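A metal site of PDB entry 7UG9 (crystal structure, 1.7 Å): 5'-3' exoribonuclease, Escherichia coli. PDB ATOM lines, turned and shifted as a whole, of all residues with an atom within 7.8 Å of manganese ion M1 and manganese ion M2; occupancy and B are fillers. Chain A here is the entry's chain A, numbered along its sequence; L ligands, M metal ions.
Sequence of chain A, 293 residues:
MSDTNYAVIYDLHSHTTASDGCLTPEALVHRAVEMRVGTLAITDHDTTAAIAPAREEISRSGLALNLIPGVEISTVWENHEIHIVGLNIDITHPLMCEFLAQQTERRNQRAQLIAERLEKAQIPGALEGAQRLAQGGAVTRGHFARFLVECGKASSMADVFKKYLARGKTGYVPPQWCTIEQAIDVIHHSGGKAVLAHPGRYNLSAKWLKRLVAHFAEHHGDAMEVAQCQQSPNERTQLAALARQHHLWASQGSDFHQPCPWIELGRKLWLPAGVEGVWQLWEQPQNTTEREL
OH of Tyr 202 is in hydrogen-bond range of N of His 83, at 2.9 Å. The side-chain carboxylate of Asp 255 lies within salt-bridge range of the guanidinium group of Arg 201, at 3.1 Å. A ring nitrogen (ND1) of His 15 is in hydrogen-bond range of the side-chain hydroxyl (OG) of Ser 19 (3.1 Å). The side-chain carboxylate of Glu 225 is in hydrogen-bond range of a ring nitrogen (ND1) of His 13 (2.7 Å). A ring nitrogen (ND1) of His 198 lies close to the side-chain hydroxyl of Tyr 202. NE2 of His 83 lies within hydrogen-bond range of OE2 of Glu 81, at 2.7 Å. The backbone NH (N) of His 15 lies within hydrogen-bond range of the backbone carbonyl oxygen (O) of Phe 256 (2.9 Å). N of Ala 197 is in hydrogen-bond range of O of His 83, 3.0 Å away.
Within 4 Å of manganese ion M1: His 13, His 15, Glu 72 and Asp 255.
NH2 of Arg 201 touches manganese ion M2, 3.98 Å away. Within 4 Å of manganese ion M2: Glu 72, His 83, His 198 and Arg 201.
Manganese ion M1 is bound by O2 of the ligand, NE2 of His 15, NE2 of His 13, OE1 of Glu 72, OD1 of Asp 255 and O3 of the ligand. Manganese ion M1 has six donor atoms within binding distance.
The side-chain carboxylate (OE2) of Glu 72 binds manganese ion M2 (2.0 Å). Manganese ion M2 is bound by a ring nitrogen (NE2) of His 198 (2.1 Å). ND1 of His 83 binds manganese ion M2 (2.1 Å). Manganese ion M2 is bound by O2 of the ligand, 2.1 Å away. Manganese ion M2 is bound by an oxygen (O1) of the ligand (2.4 Å).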
ATOM      1  N   HIS A  13      -9.267  25.048  -6.166  1.00  0.00           N
ATOM      2  CA  HIS A  13      -9.412  23.602  -6.283  1.00  0.00           C
ATOM      3  C   HIS A  13      -8.008  22.996  -6.248  1.00  0.00           C
ATOM      4  O   HIS A  13      -7.271  23.136  -7.219  1.00  0.00           O
ATOM      5  CB  HIS A  13     -10.147  23.227  -7.562  1.00  0.00           C
ATOM      6  CG  HIS A  13     -10.625  21.797  -7.600  1.00  0.00           C
ATOM      7  ND1 HIS A  13     -11.831  21.439  -8.158  1.00  0.00           N
ATOM      8  CD2 HIS A  13     -10.050  20.648  -7.167  1.00  0.00           C
ATOM      9  CE1 HIS A  13     -11.973  20.124  -8.082  1.00  0.00           C
ATOM     10  NE2 HIS A  13     -10.916  19.614  -7.479  1.00  0.00           N
ATOM     11  N   SER A  14      -7.661  22.346  -5.141  1.00  0.00           N
ATOM     12  CA  SER A  14      -6.326  21.749  -5.012  1.00  0.00           C
ATOM     13  C   SER A  14      -6.380  20.612  -4.007  1.00  0.00           C
ATOM     14  O   SER A  14      -7.291  20.546  -3.160  1.00  0.00           O
ATOM     15  CB  SER A  14      -5.292  22.789  -4.551  1.00  0.00           C
ATOM     16  OG  SER A  14      -5.610  23.257  -3.247  1.00  0.00           O
ATOM     17  N   HIS A  15      -5.397  19.718  -4.095  1.00  0.00           N
ATOM     18  CA  HIS A  15      -5.349  18.524  -3.249  1.00  0.00           C
ATOM     19  C   HIS A  15      -4.003  18.396  -2.548  1.00  0.00           C
ATOM     20  O   HIS A  15      -2.990  18.925  -3.008  1.00  0.00           O
ATOM     21  CB  HIS A  15      -5.600  17.251  -4.056  1.00  0.00           C
ATOM     22  CG  HIS A  15      -6.974  17.202  -4.626  1.00  0.00           C
ATOM     23  ND1 HIS A  15      -7.975  16.472  -4.039  1.00  0.00           N
ATOM     24  CD2 HIS A  15      -7.504  17.762  -5.731  1.00  0.00           C
ATOM     25  CE1 HIS A  15      -9.090  16.618  -4.743  1.00  0.00           C
ATOM     26  NE2 HIS A  15      -8.832  17.394  -5.771  1.00  0.00           N
ATOM     27  N   SER A  19      -5.819  13.809   0.853  1.00  0.00           N
ATOM     28  CA  SER A  19      -6.540  12.923  -0.062  1.00  0.00           C
ATOM     29  C   SER A  19      -5.555  12.356  -1.064  1.00  0.00           C
ATOM     30  O   SER A  19      -4.648  11.607  -0.689  1.00  0.00           O
ATOM     31  CB  SER A  19      -7.742  13.629  -0.722  1.00  0.00           C
ATOM     32  OG  SER A  19      -7.425  14.669  -1.614  1.00  0.00           O
ATOM     33  N   ASP A  20      -5.664  12.716  -2.342  1.00  0.00           N
ATOM     34  CA  ASP A  20      -4.821  12.052  -3.339  1.00  0.00           C
ATOM     35  C   ASP A  20      -3.768  12.984  -3.941  1.00  0.00           C
ATOM     36  O   ASP A  20      -3.272  12.701  -5.029  1.00  0.00           O
ATOM     37  CB  ASP A  20      -5.670  11.409  -4.437  1.00  0.00           C
ATOM     38  CG  ASP A  20      -6.573  12.394  -5.163  1.00  0.00           C
ATOM     39  OD1 ASP A  20      -6.695  13.548  -4.700  1.00  0.00           O
ATOM     40  OD2 ASP A  20      -7.159  12.015  -6.193  1.00  0.00           O
ATOM     41  N   THR A  43      -9.221  21.556  -1.406  1.00  0.00           N
ATOM     42  CA  THR A  43     -10.497  20.885  -1.651  1.00  0.00           C
ATOM     43  C   THR A  43     -10.241  19.372  -1.768  1.00  0.00           C
ATOM     44  O   THR A  43     -10.469  18.761  -2.807  1.00  0.00           O
ATOM     45  CB  THR A  43     -11.184  21.448  -2.901  1.00  0.00           C
ATOM     46  OG1 THR A  43     -10.385  21.240  -4.081  1.00  0.00           O
ATOM     47  CG2 THR A  43     -11.466  22.964  -2.745  1.00  0.00           C
ATOM     48  N   ASP A  44      -9.764  18.769  -0.681  1.00  0.00           N
ATOM     49  CA  ASP A  44      -9.462  17.342  -0.672  1.00  0.00           C
ATOM     50  C   ASP A  44     -10.754  16.519  -0.770  1.00  0.00           C
ATOM     51  O   ASP A  44     -11.820  16.967  -0.375  1.00  0.00           O
ATOM     52  CB  ASP A  44      -8.670  16.995   0.589  1.00  0.00           C
ATOM     53  CG  ASP A  44      -7.164  17.241   0.434  1.00  0.00           C
ATOM     54  OD1 ASP A  44      -6.594  16.860  -0.614  1.00  0.00           O
ATOM     55  OD2 ASP A  44      -6.572  17.921   1.302  1.00  0.00           O
ATOM     56  N   HIS A  45     -10.635  15.309  -1.335  1.00  0.00           N
ATOM     57  CA  HIS A  45     -11.780  14.409  -1.460  1.00  0.00           C
ATOM     58  C   HIS A  45     -12.337  14.006  -0.114  1.00  0.00           C
ATOM     59  O   HIS A  45     -11.676  13.301   0.661  1.00  0.00           O
ATOM     60  CB  HIS A  45     -11.384  13.151  -2.244  1.00  0.00           C
ATOM     61  CG  HIS A  45     -10.976  13.418  -3.653  1.00  0.00           C
ATOM     62  ND1 HIS A  45     -11.876  13.781  -4.625  1.00  0.00           N
ATOM     63  CD2 HIS A  45      -9.767  13.364  -4.253  1.00  0.00           C
ATOM     64  CE1 HIS A  45     -11.240  13.937  -5.774  1.00  0.00           C
ATOM     65  NE2 HIS A  45      -9.952  13.719  -5.572  1.00  0.00           N
ATOM     66  N   GLU A  72     -13.946  18.503  -1.570  1.00  0.00           N
ATOM     67  CA  GLU A  72     -14.526  17.988  -2.808  1.00  0.00           C
ATOM     68  C   GLU A  72     -15.353  16.759  -2.483  1.00  0.00           C
ATOM     69  O   GLU A  72     -14.819  15.764  -1.991  1.00  0.00           O
ATOM     70  CB  GLU A  72     -13.451  17.663  -3.841  1.00  0.00           C
ATOM     71  CG  GLU A  72     -14.124  17.408  -5.219  1.00  0.00           C
ATOM     72  CD  GLU A  72     -13.158  17.189  -6.342  1.00  0.00           C
ATOM     73  OE1 GLU A  72     -11.950  17.070  -6.062  1.00  0.00           O
ATOM     74  OE2 GLU A  72     -13.603  17.227  -7.516  1.00  0.00           O
ATOM     75  N   ILE A  73     -16.664  16.822  -2.773  1.00  0.00           N
ATOM     76  CA  ILE A  73     -17.624  15.777  -2.409  1.00  0.00           C
ATOM     77  C   ILE A  73     -17.987  14.975  -3.639  1.00  0.00           C
ATOM     78  O   ILE A  73     -18.251  15.541  -4.711  1.00  0.00           O
ATOM     79  CB  ILE A  73     -18.883  16.422  -1.786  1.00  0.00           C
ATOM     80  CG1 ILE A  73     -18.487  17.169  -0.523  1.00  0.00           C
ATOM     81  CG2 ILE A  73     -19.942  15.357  -1.493  1.00  0.00           C
ATOM     82  CD1 ILE A  73     -19.639  17.962   0.129  1.00  0.00           C
ATOM     83  N   SER A  74     -18.002  13.655  -3.510  1.00  0.00           N
ATOM     84  CA  SER A  74     -18.322  12.763  -4.611  1.00  0.00           C
ATOM     85  C   SER A  74     -19.822  12.457  -4.573  1.00  0.00           C
ATOM     86  O   SER A  74     -20.335  12.022  -3.541  1.00  0.00           O
ATOM     87  CB  SER A  74     -17.491  11.483  -4.490  1.00  0.00           C
ATOM     88  OG  SER A  74     -16.107  11.807  -4.481  1.00  0.00           O
ATOM     89  N   GLU A  81     -20.873   9.894 -11.992  1.00  0.00           N
ATOM     90  CA  GLU A  81     -20.151  10.439 -10.846  1.00  0.00           C
ATOM     91  C   GLU A  81     -19.913  11.934 -11.070  1.00  0.00           C
ATOM     92  O   GLU A  81     -19.296  12.334 -12.075  1.00  0.00           O
ATOM     93  CB  GLU A  81     -18.820   9.717 -10.638  1.00  0.00           C
ATOM     94  CG  GLU A  81     -18.008  10.346  -9.510  1.00  0.00           C
ATOM     95  CD  GLU A  81     -16.834   9.484  -9.077  1.00  0.00           C
ATOM     96  OE1 GLU A  81     -16.837   8.274  -9.385  1.00  0.00           O
ATOM     97  OE2 GLU A  81     -15.933  10.025  -8.393  1.00  0.00           O
ATOM     98  N   ILE A  82     -20.402  12.761 -10.166  1.00  0.00           N
ATOM     99  CA  ILE A  82     -20.281  14.207 -10.267  1.00  0.00           C
ATOM    100  C   ILE A  82     -19.617  14.701  -9.004  1.00  0.00           C
ATOM    101  O   ILE A  82     -19.922  14.222  -7.904  1.00  0.00           O
ATOM    102  CB  ILE A  82     -21.670  14.893 -10.443  1.00  0.00           C
ATOM    103  CG1 ILE A  82     -22.411  14.335 -11.665  1.00  0.00           C
ATOM    104  CG2 ILE A  82     -21.513  16.399 -10.594  1.00  0.00           C
ATOM    105  CD1 ILE A  82     -21.705  14.642 -13.024  1.00  0.00           C
ATOM    106  N   HIS A  83     -18.702  15.653  -9.139  1.00  0.00           N
ATOM    107  CA  HIS A  83     -17.972  16.194  -8.007  1.00  0.00           C
ATOM    108  C   HIS A  83     -18.469  17.602  -7.694  1.00  0.00           C
ATOM    109  O   HIS A  83     -18.548  18.445  -8.590  1.00  0.00           O
ATOM    110  CB  HIS A  83     -16.452  16.204  -8.277  1.00  0.00           C
ATOM    111  CG  HIS A  83     -15.848  14.829  -8.361  1.00  0.00           C
ATOM    112  ND1 HIS A  83     -14.578  14.588  -8.844  1.00  0.00           N
ATOM    113  CD2 HIS A  83     -16.365  13.608  -8.053  1.00  0.00           C
ATOM    114  CE1 HIS A  83     -14.321  13.285  -8.803  1.00  0.00           C
ATOM    115  NE2 HIS A  83     -15.392  12.675  -8.314  1.00  0.00           N
ATOM    116  N   ILE A  84     -18.785  17.840  -6.431  1.00  0.00           N
ATOM    117  CA  ILE A  84     -19.243  19.129  -5.936  1.00  0.00           C
ATOM    118  C   ILE A  84     -18.226  19.617  -4.934  1.00  0.00           C
ATOM    119  O   ILE A  84     -17.870  18.883  -4.004  1.00  0.00           O
ATOM    120  CB  ILE A  84     -20.639  19.035  -5.275  1.00  0.00           C
ATOM    121  CG1 ILE A  84     -21.650  18.340  -6.200  1.00  0.00           C
ATOM    122  CG2 ILE A  84     -21.129  20.389  -4.808  1.00  0.00           C
ATOM    123  CD1 ILE A  84     -21.978  19.150  -7.425  1.00  0.00           C
ATOM    124  N   VAL A  85     -17.728  20.824  -5.133  1.00  0.00           N
ATOM    125  CA  VAL A  85     -16.751  21.422  -4.237  1.00  0.00           C
ATOM    126  C   VAL A  85     -17.527  22.342  -3.295  1.00  0.00           C
ATOM    127  O   VAL A  85     -18.431  23.046  -3.732  1.00  0.00           O
ATOM    128  CB  VAL A  85     -15.692  22.194  -5.026  1.00  0.00           C
ATOM    129  CG1 VAL A  85     -14.891  23.123  -4.117  1.00  0.00           C
ATOM    130  CG2 VAL A  85     -14.750  21.207  -5.733  1.00  0.00           C
ATOM    131  N   ALA A 197     -17.908  21.078  -9.948  1.00  0.00           N
ATOM    132  CA  ALA A 197     -16.503  20.999 -10.328  1.00  0.00           C
ATOM    133  C   ALA A 197     -16.329  20.491 -11.744  1.00  0.00           C
ATOM    134  O   ALA A 197     -17.111  19.667 -12.234  1.00  0.00           O
ATOM    135  CB  ALA A 197     -15.764  20.080  -9.371  1.00  0.00           C
ATOM    136  N   HIS A 198     -15.239  20.963 -12.397  1.00  0.00           N
ATOM    137  CA  HIS A 198     -14.719  20.576 -13.710  1.00  0.00           C
ATOM    138  C   HIS A 198     -15.816  20.025 -14.612  1.00  0.00           C
ATOM    139  O   HIS A 198     -15.822  18.836 -14.955  1.00  0.00           O
ATOM    140  CB  HIS A 198     -13.551  19.575 -13.578  1.00  0.00           C
ATOM    141  CG  HIS A 198     -13.730  18.514 -12.527  1.00  0.00           C
ATOM    142  ND1 HIS A 198     -14.670  17.517 -12.613  1.00  0.00           N
ATOM    143  CD2 HIS A 198     -13.030  18.280 -11.390  1.00  0.00           C
ATOM    144  CE1 HIS A 198     -14.582  16.732 -11.557  1.00  0.00           C
ATOM    145  NE2 HIS A 198     -13.583  17.163 -10.796  1.00  0.00           N
ATOM    146  N   ARG A 201     -15.087  17.773 -17.740  1.00  0.00           N
ATOM    147  CA  ARG A 201     -14.526  16.426 -17.583  1.00  0.00           C
ATOM    148  C   ARG A 201     -15.568  15.336 -17.573  1.00  0.00           C
ATOM    149  O   ARG A 201     -15.215  14.156 -17.680  1.00  0.00           O
ATOM    150  CB  ARG A 201     -13.697  16.328 -16.299  1.00  0.00           C
ATOM    151  CG  ARG A 201     -12.248  16.664 -16.522  1.00  0.00           C
ATOM    152  CD  ARG A 201     -11.337  16.271 -15.359  1.00  0.00           C
ATOM    153  NE  ARG A 201     -11.872  15.270 -14.445  1.00  0.00           N
ATOM    154  CZ  ARG A 201     -11.413  15.108 -13.217  1.00  0.00           C
ATOM    155  NH1 ARG A 201     -10.442  15.857 -12.744  1.00  0.00           N
ATOM    156  NH2 ARG A 201     -11.961  14.177 -12.423  1.00  0.00           N
ATOM    157  N   TYR A 202     -16.857  15.666 -17.444  1.00  0.00           N
ATOM    158  CA  TYR A 202     -17.832  14.604 -17.390  1.00  0.00           C
ATOM    159  C   TYR A 202     -18.159  14.087 -18.782  1.00  0.00           C
ATOM    160  O   TYR A 202     -18.893  13.098 -18.909  1.00  0.00           O
ATOM    161  CB  TYR A 202     -19.093  15.104 -16.676  1.00  0.00           C
ATOM    162  CG  TYR A 202     -18.805  15.643 -15.278  1.00  0.00           C
ATOM    163  CD1 TYR A 202     -18.047  14.914 -14.353  1.00  0.00           C
ATOM    164  CD2 TYR A 202     -19.229  16.918 -14.923  1.00  0.00           C
ATOM    165  CE1 TYR A 202     -17.784  15.412 -13.081  1.00  0.00           C
ATOM    166  CE2 TYR A 202     -18.958  17.434 -13.664  1.00  0.00           C
ATOM    167  CZ  TYR A 202     -18.232  16.670 -12.755  1.00  0.00           C
ATOM    168  OH  TYR A 202     -17.972  17.183 -11.509  1.00  0.00           O
ATOM    169  N   GLU A 225     -17.260  25.678 -11.756  1.00  0.00           N
ATOM    170  CA  GLU A 225     -15.896  25.934 -12.191  1.00  0.00           C
ATOM    171  C   GLU A 225     -15.909  26.232 -13.677  1.00  0.00           C
ATOM    172  O   GLU A 225     -16.455  25.467 -14.483  1.00  0.00           O
ATOM    173  CB  GLU A 225     -14.993  24.736 -11.879  1.00  0.00           C
ATOM    174  CG  GLU A 225     -14.747  24.622 -10.403  1.00  0.00           C
ATOM    175  CD  GLU A 225     -13.784  23.508 -10.025  1.00  0.00           C
ATOM    176  OE1 GLU A 225     -13.391  22.690 -10.890  1.00  0.00           O
ATOM    177  OE2 GLU A 225     -13.418  23.466  -8.834  1.00  0.00           O
ATOM    178  N   SER A 254      -7.095  24.833 -10.328  1.00  0.00           N
ATOM    179  CA  SER A 254      -6.168  24.021 -11.095  1.00  0.00           C
ATOM    180  C   SER A 254      -6.445  22.539 -10.951  1.00  0.00           C
ATOM    181  O   SER A 254      -6.032  21.757 -11.821  1.00  0.00           O
ATOM    182  CB  SER A 254      -4.725  24.291 -10.659  1.00  0.00           C
ATOM    183  OG  SER A 254      -4.560  24.067  -9.262  1.00  0.00           O
ATOM    184  N   ASP A 255      -7.102  22.126  -9.857  1.00  0.00           N
ATOM    185  CA  ASP A 255      -7.214  20.719  -9.502  1.00  0.00           C
ATOM    186  C   ASP A 255      -5.836  20.102  -9.343  1.00  0.00           C
ATOM    187  O   ASP A 255      -5.585  18.968  -9.738  1.00  0.00           O
ATOM    188  CB  ASP A 255      -8.018  19.951 -10.549  1.00  0.00           C
ATOM    189  CG  ASP A 255      -8.640  18.701 -10.014  1.00  0.00           C
ATOM    190  OD1 ASP A 255      -8.518  18.417  -8.810  1.00  0.00           O
ATOM    191  OD2 ASP A 255      -9.227  17.954 -10.828  1.00  0.00           O
ATOM    192  N   PHE A 256      -4.925  20.887  -8.784  1.00  0.00           N
ATOM    193  CA  PHE A 256      -3.552  20.426  -8.593  1.00  0.00           C
ATOM    194  C   PHE A 256      -3.487  19.206  -7.683  1.00  0.00           C
ATOM    195  O   PHE A 256      -4.015  19.215  -6.577  1.00  0.00           O
ATOM    196  CB  PHE A 256      -2.733  21.570  -8.002  1.00  0.00           C
ATOM    197  CG  PHE A 256      -1.315  21.203  -7.701  1.00  0.00           C
ATOM    198  CD1 PHE A 256      -0.964  20.641  -6.486  1.00  0.00           C
ATOM    199  CD2 PHE A 256      -0.333  21.426  -8.651  1.00  0.00           C
ATOM    200  CE1 PHE A 256       0.370  20.309  -6.215  1.00  0.00           C
ATOM    201  CE2 PHE A 256       0.982  21.131  -8.379  1.00  0.00           C
ATOM    202  CZ  PHE A 256       1.323  20.546  -7.164  1.00  0.00           C
ATOM    203  N   HIS A 257      -2.769  18.178  -8.146  1.00  0.00           N
ATOM    204  CA  HIS A 257      -2.422  17.011  -7.328  1.00  0.00           C
ATOM    205  C   HIS A 257      -0.920  16.881  -7.108  1.00  0.00           C
ATOM    206  O   HIS A 257      -0.485  16.614  -5.997  1.00  0.00           O
ATOM    207  CB  HIS A 257      -2.918  15.716  -7.982  1.00  0.00           C
ATOM    208  CG  HIS A 257      -4.392  15.524  -7.905  1.00  0.00           C
ATOM    209  ND1 HIS A 257      -5.283  16.322  -8.590  1.00  0.00           N
ATOM    210  CD2 HIS A 257      -5.149  14.584  -7.268  1.00  0.00           C
ATOM    211  CE1 HIS A 257      -6.512  15.910  -8.364  1.00  0.00           C
ATOM    212  NE2 HIS A 257      -6.464  14.870  -7.544  1.00  0.00           N
HETATM  213  S1  LIG L   1     -10.347  15.233  -9.168  1.00  0.00           S
HETATM  214  O1  LIG L   1     -11.449  14.276  -9.260  1.00  0.00           O
HETATM  215  O2  LIG L   1     -10.998  16.539  -9.038  1.00  0.00           O
HETATM  216  O3  LIG L   1      -9.484  15.057  -8.013  1.00  0.00           O
HETATM  217  O4  LIG L   1      -9.529  15.179 -10.377  1.00  0.00           O
HETATM  218 MN    MN M   1     -10.212  17.568  -7.395  1.00  0.00          MN
HETATM  219 MN    MN M   2     -13.063  16.048  -9.083  1.00  0.00          MN
HETATM  220 MN    MN M   3      -8.228  13.737  -6.973  1.00  0.00          MN
